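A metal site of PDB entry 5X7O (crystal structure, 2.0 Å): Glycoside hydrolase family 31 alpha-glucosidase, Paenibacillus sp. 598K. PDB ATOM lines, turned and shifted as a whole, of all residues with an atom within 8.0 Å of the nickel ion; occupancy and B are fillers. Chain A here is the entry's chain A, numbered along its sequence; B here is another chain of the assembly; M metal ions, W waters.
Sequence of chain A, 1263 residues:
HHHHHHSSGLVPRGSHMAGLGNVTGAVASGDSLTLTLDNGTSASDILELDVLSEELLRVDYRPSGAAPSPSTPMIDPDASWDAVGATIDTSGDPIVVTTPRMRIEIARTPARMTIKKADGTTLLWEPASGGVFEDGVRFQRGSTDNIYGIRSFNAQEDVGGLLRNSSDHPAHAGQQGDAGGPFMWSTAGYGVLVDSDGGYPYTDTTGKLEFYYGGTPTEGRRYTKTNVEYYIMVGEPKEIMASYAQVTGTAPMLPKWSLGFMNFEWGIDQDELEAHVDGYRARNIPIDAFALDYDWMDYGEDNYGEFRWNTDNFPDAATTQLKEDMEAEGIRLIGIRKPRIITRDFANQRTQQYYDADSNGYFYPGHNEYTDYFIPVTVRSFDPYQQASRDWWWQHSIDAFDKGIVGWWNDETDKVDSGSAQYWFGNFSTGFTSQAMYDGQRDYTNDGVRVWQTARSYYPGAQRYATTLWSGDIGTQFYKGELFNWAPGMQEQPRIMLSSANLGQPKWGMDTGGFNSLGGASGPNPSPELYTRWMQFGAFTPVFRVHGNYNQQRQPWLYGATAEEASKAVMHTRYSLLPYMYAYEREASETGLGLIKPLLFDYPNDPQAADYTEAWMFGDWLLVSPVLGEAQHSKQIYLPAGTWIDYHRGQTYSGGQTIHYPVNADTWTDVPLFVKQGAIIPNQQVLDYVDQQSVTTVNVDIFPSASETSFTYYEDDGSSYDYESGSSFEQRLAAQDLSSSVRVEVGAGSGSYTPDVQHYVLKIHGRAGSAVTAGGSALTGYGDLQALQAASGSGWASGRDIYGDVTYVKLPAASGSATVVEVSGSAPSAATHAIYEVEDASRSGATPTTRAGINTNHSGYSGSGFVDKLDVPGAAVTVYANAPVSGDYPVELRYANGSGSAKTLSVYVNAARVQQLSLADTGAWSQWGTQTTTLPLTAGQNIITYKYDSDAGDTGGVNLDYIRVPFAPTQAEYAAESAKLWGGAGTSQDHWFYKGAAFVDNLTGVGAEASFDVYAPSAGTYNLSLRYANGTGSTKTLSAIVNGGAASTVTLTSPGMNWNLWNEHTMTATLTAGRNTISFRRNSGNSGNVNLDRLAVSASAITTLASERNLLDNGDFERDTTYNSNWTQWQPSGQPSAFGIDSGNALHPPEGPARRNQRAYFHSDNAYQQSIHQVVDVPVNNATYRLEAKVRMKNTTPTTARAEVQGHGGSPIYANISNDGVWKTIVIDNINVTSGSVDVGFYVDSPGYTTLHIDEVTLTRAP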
ATOM      1  N   ILE A 150      33.727 -18.870 -18.621  1.00  0.00           N
ATOM      2  CA  ILE A 150      33.677 -17.437 -18.263  1.00  0.00           C
ATOM      3  C   ILE A 150      32.828 -17.128 -17.031  1.00  0.00           C
ATOM      4  O   ILE A 150      33.317 -16.471 -16.121  1.00  0.00           O
ATOM      5  CB  ILE A 150      33.214 -16.530 -19.443  1.00  0.00           C
ATOM      6  CG1 ILE A 150      34.181 -16.603 -20.613  1.00  0.00           C
ATOM      7  CG2 ILE A 150      33.101 -15.093 -18.985  1.00  0.00           C
ATOM      8  CD1 ILE A 150      33.624 -16.010 -21.917  1.00  0.00           C
ATOM      9  N   ARG A 151      31.565 -17.534 -17.049  1.00  0.00           N
ATOM     10  CA  ARG A 151      30.582 -17.050 -16.077  1.00  0.00           C
ATOM     11  C   ARG A 151      29.424 -18.003 -15.881  1.00  0.00           C
ATOM     12  O   ARG A 151      29.103 -18.787 -16.762  1.00  0.00           O
ATOM     13  CB  ARG A 151      30.060 -15.668 -16.497  1.00  0.00           C
ATOM     14  CG  ARG A 151      29.326 -15.585 -17.843  1.00  0.00           C
ATOM     15  CD  ARG A 151      27.818 -15.838 -17.755  1.00  0.00           C
ATOM     16  NE  ARG A 151      27.108 -14.874 -16.904  1.00  0.00           N
ATOM     17  CZ  ARG A 151      26.624 -13.695 -17.284  1.00  0.00           C
ATOM     18  NH1 ARG A 151      26.767 -13.232 -18.536  1.00  0.00           N
ATOM     19  NH2 ARG A 151      25.975 -12.942 -16.409  1.00  0.00           N
ATOM     20  N   SER A 152      28.776 -17.875 -14.716  1.00  0.00           N
ATOM     21  CA  SER A 152      27.490 -18.492 -14.438  1.00  0.00           C
ATOM     22  C   SER A 152      26.463 -17.394 -14.122  1.00  0.00           C
ATOM     23  O   SER A 152      26.588 -16.262 -14.598  1.00  0.00           O
ATOM     24  CB  SER A 152      27.658 -19.494 -13.303  1.00  0.00           C
ATOM     25  OG  SER A 152      26.437 -20.184 -13.068  1.00  0.00           O
ATOM     26  N   PHE A 153      25.433 -17.703 -13.324  1.00  0.00           N
ATOM     27  CA  PHE A 153      24.405 -16.714 -12.988  1.00  0.00           C
ATOM     28  C   PHE A 153      24.069 -16.742 -11.512  1.00  0.00           C
ATOM     29  O   PHE A 153      24.035 -17.816 -10.909  1.00  0.00           O
ATOM     30  CB  PHE A 153      23.160 -16.929 -13.845  1.00  0.00           C
ATOM     31  CG  PHE A 153      23.455 -16.942 -15.306  1.00  0.00           C
ATOM     32  CD1 PHE A 153      23.527 -15.746 -16.034  1.00  0.00           C
ATOM     33  CD2 PHE A 153      23.714 -18.137 -15.962  1.00  0.00           C
ATOM     34  CE1 PHE A 153      23.834 -15.753 -17.386  1.00  0.00           C
ATOM     35  CE2 PHE A 153      24.012 -18.142 -17.316  1.00  0.00           C
ATOM     36  CZ  PHE A 153      24.077 -16.951 -18.027  1.00  0.00           C
ATOM     37  N   ASN A 154      23.843 -15.572 -10.919  1.00  0.00           N
ATOM     38  CA  ASN A 154      23.551 -15.480  -9.487  1.00  0.00           C
ATOM     39  C   ASN A 154      22.044 -15.529  -9.205  1.00  0.00           C
ATOM     40  O   ASN A 154      21.239 -15.523 -10.129  1.00  0.00           O
ATOM     41  CB  ASN A 154      24.272 -14.299  -8.803  1.00  0.00           C
ATOM     42  CG  ASN A 154      23.744 -12.918  -9.168  1.00  0.00           C
ATOM     43  OD1 ASN A 154      22.557 -12.706  -9.447  1.00  0.00           O
ATOM     44  ND2 ASN A 154      24.645 -11.938  -9.112  1.00  0.00           N
ATOM     45  N   GLU A 157      19.845 -12.413 -10.694  1.00  0.00           N
ATOM     46  CA  GLU A 157      20.120 -12.082 -12.093  1.00  0.00           C
ATOM     47  C   GLU A 157      19.166 -12.830 -12.994  1.00  0.00           C
ATOM     48  O   GLU A 157      18.698 -13.905 -12.634  1.00  0.00           O
ATOM     49  CB  GLU A 157      21.544 -12.556 -12.485  1.00  0.00           C
ATOM     50  CG  GLU A 157      22.605 -11.498 -12.357  1.00  0.00           C
ATOM     51  CD  GLU A 157      24.023 -11.991 -12.678  1.00  0.00           C
ATOM     52  OE1 GLU A 157      24.313 -13.226 -12.661  1.00  0.00           O
ATOM     53  OE2 GLU A 157      24.851 -11.107 -12.958  1.00  0.00           O
ATOM     54  N   HIS A 169      30.840 -10.130 -20.141  1.00  0.00           N
ATOM     55  CA  HIS A 169      30.735 -10.178 -18.687  1.00  0.00           C
ATOM     56  C   HIS A 169      32.133 -10.384 -18.088  1.00  0.00           C
ATOM     57  O   HIS A 169      32.876 -11.169 -18.626  1.00  0.00           O
ATOM     58  CB  HIS A 169      29.799 -11.347 -18.309  1.00  0.00           C
ATOM     59  CG  HIS A 169      29.333 -11.330 -16.897  1.00  0.00           C
ATOM     60  ND1 HIS A 169      28.335 -10.481 -16.459  1.00  0.00           N
ATOM     61  CD2 HIS A 169      29.688 -12.085 -15.837  1.00  0.00           C
ATOM     62  CE1 HIS A 169      28.127 -10.689 -15.171  1.00  0.00           C
ATOM     63  NE2 HIS A 169      28.928 -11.669 -14.770  1.00  0.00           N
ATOM     64  N   PRO A 170      32.511  -9.686 -16.985  1.00  0.00           N
ATOM     65  CA  PRO A 170      33.833  -9.945 -16.379  1.00  0.00           C
ATOM     66  C   PRO A 170      33.988 -11.341 -15.792  1.00  0.00           C
ATOM     67  O   PRO A 170      32.977 -12.032 -15.559  1.00  0.00           O
ATOM     68  CB  PRO A 170      33.933  -8.910 -15.248  1.00  0.00           C
ATOM     69  CG  PRO A 170      32.777  -7.967 -15.438  1.00  0.00           C
ATOM     70  CD  PRO A 170      31.728  -8.726 -16.189  1.00  0.00           C
ATOM     71  N   ALA A 171      35.240 -11.732 -15.569  1.00  0.00           N
ATOM     72  CA  ALA A 171      35.586 -12.969 -14.880  1.00  0.00           C
ATOM     73  C   ALA A 171      35.693 -12.616 -13.405  1.00  0.00           C
ATOM     74  O   ALA A 171      36.512 -11.796 -13.017  1.00  0.00           O
ATOM     75  CB  ALA A 171      36.920 -13.526 -15.395  1.00  0.00           C
ATOM     76  N   HIS A 172      34.822 -13.210 -12.590  1.00  0.00           N
ATOM     77  CA  HIS A 172      34.823 -12.973 -11.154  1.00  0.00           C
ATOM     78  C   HIS A 172      34.138 -14.117 -10.420  1.00  0.00           C
ATOM     79  O   HIS A 172      33.359 -14.863 -11.028  1.00  0.00           O
ATOM     80  CB  HIS A 172      34.158 -11.620 -10.790  1.00  0.00           C
ATOM     81  CG  HIS A 172      32.757 -11.429 -11.326  1.00  0.00           C
ATOM     82  ND1 HIS A 172      32.362 -10.260 -11.934  1.00  0.00           N
ATOM     83  CD2 HIS A 172      31.666 -12.230 -11.313  1.00  0.00           C
ATOM     84  CE1 HIS A 172      31.081 -10.352 -12.287  1.00  0.00           C
ATOM     85  NE2 HIS A 172      30.639 -11.536 -11.918  1.00  0.00           N
ATOM     86  N   ALA A 173      34.446 -14.271  -9.133  1.00  0.00           N
ATOM     87  CA  ALA A 173      33.694 -15.178  -8.269  1.00  0.00           C
ATOM     88  C   ALA A 173      32.226 -14.772  -8.135  1.00  0.00           C
ATOM     89  O   ALA A 173      31.362 -15.632  -8.101  1.00  0.00           O
ATOM     90  CB  ALA A 173      34.331 -15.263  -6.896  1.00  0.00           C
ATOM     91  N   GLY A 174      31.964 -13.471  -8.060  1.00  0.00           N
ATOM     92  CA  GLY A 174      30.600 -12.928  -7.962  1.00  0.00           C
ATOM     93  C   GLY A 174      29.994 -13.187  -6.589  1.00  0.00           C
ATOM     94  O   GLY A 174      30.706 -13.400  -5.603  1.00  0.00           O
ATOM     95  N   GLN A 175      28.666 -13.170  -6.526  1.00  0.00           N
ATOM     96  CA  GLN A 175      27.952 -13.384  -5.253  1.00  0.00           C
ATOM     97  C   GLN A 175      26.725 -14.261  -5.459  1.00  0.00           C
ATOM     98  O   GLN A 175      26.320 -14.497  -6.590  1.00  0.00           O
ATOM     99  CB  GLN A 175      27.520 -12.038  -4.655  1.00  0.00           C
ATOM    100  CG  GLN A 175      26.577 -11.246  -5.556  1.00  0.00           C
ATOM    101  CD  GLN A 175      25.971 -10.023  -4.892  1.00  0.00           C
ATOM    102  OE1 GLN A 175      25.593 -10.066  -3.724  1.00  0.00           O
ATOM    103  NE2 GLN A 175      25.849  -8.944  -5.662  1.00  0.00           N
ATOM    104  N   GLY A 177      25.696 -17.397  -5.442  1.00  0.00           N
ATOM    105  CA  GLY A 177      25.690 -18.581  -6.299  1.00  0.00           C
ATOM    106  C   GLY A 177      26.401 -18.454  -7.625  1.00  0.00           C
ATOM    107  O   GLY A 177      26.486 -19.432  -8.363  1.00  0.00           O
ATOM    108  N   ASP A 178      26.910 -17.278  -7.934  1.00  0.00           N
ATOM    109  CA  ASP A 178      27.679 -17.052  -9.157  1.00  0.00           C
ATOM    110  C   ASP A 178      28.985 -17.844  -9.136  1.00  0.00           C
ATOM    111  O   ASP A 178      29.451 -18.336  -8.100  1.00  0.00           O
ATOM    112  CB  ASP A 178      27.980 -15.568  -9.302  1.00  0.00           C
ATOM    113  CG  ASP A 178      28.108 -15.089 -10.738  1.00  0.00           C
ATOM    114  OD1 ASP A 178      28.163 -15.892 -11.713  1.00  0.00           O
ATOM    115  OD2 ASP A 178      28.188 -13.842 -10.865  1.00  0.00           O
ATOM    116  N   ALA A 179      29.561 -17.965 -10.308  1.00  0.00           N
ATOM    117  CA  ALA A 179      30.855 -18.591 -10.488  1.00  0.00           C
ATOM    118  C   ALA A 179      31.414 -17.952 -11.741  1.00  0.00           C
ATOM    119  O   ALA A 179      30.659 -17.503 -12.609  1.00  0.00           O
ATOM    120  CB  ALA A 179      30.693 -20.087 -10.696  1.00  0.00           C
ATOM    121  N   GLY A 180      32.721 -17.911 -11.850  1.00  0.00           N
ATOM    122  CA  GLY A 180      33.345 -17.394 -13.060  1.00  0.00           C
ATOM    123  C   GLY A 180      34.846 -17.469 -12.999  1.00  0.00           C
ATOM    124  O   GLY A 180      35.425 -17.854 -11.958  1.00  0.00           O
ATOM    125  N   TRP B 424      32.790  -5.633  -1.228  1.00  0.00           N
ATOM    126  CA  TRP B 424      33.093  -6.880  -1.939  1.00  0.00           C
ATOM    127  C   TRP B 424      34.267  -7.622  -1.298  1.00  0.00           C
ATOM    128  O   TRP B 424      35.263  -7.019  -0.907  1.00  0.00           O
ATOM    129  CB  TRP B 424      33.429  -6.607  -3.389  1.00  0.00           C
ATOM    130  CG  TRP B 424      32.264  -6.417  -4.223  1.00  0.00           C
ATOM    131  CD1 TRP B 424      31.644  -5.245  -4.493  1.00  0.00           C
ATOM    132  CD2 TRP B 424      31.552  -7.435  -4.929  1.00  0.00           C
ATOM    133  NE1 TRP B 424      30.571  -5.460  -5.334  1.00  0.00           N
ATOM    134  CE2 TRP B 424      30.500  -6.798  -5.621  1.00  0.00           C
ATOM    135  CE3 TRP B 424      31.694  -8.828  -5.040  1.00  0.00           C
ATOM    136  CZ2 TRP B 424      29.586  -7.499  -6.420  1.00  0.00           C
ATOM    137  CZ3 TRP B 424      30.785  -9.535  -5.828  1.00  0.00           C
ATOM    138  CH2 TRP B 424      29.739  -8.870  -6.509  1.00  0.00           C
HETATM  139 NI    NI M   1      28.669 -12.794 -12.720  1.00  0.00          NI
HETATM  140  O   HOH W   1      29.822 -14.560 -13.378  1.00  0.00           O
HETATM  141  O   HOH W   2      26.737 -13.651 -13.621  1.00  0.00           O
HETATM  142  O   HOH W   3      27.179 -11.305 -12.072  1.00  0.00           O
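ND1 of His 169 sits close to NH2 of Arg 151.
The backbone carbonyl oxygen of His 172 sits at hydrogen-bond distance from the backbone NH of Gly 180, at 3.2 Å.
Water W1 bridges OD1 of Asp 178 (2.7 Å) and O of Ala 179 (3.2 Å).
OD2 of Asp 178 binds the nickel ion (2.2 Å).
The nickel ion is bound by water W3, 2.2 Å away.
Water W1 binds the nickel ion (2.2 Å).
Water W2 binds the nickel ion, at 2.3 Å.
The nickel ion is bound by NE2 of His 169, at 2.4 Å.
NE2 of His 172 is bound to the nickel ion, at 2.5 Å.
The nickel ion has six donor atoms within binding distance.
Three residues have an atom within 4 Å of the nickel ion: His 169, His 172 and Asp 178.
Along chain A the residues within 4 Å of the nickel ion span positions 169 to 178.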
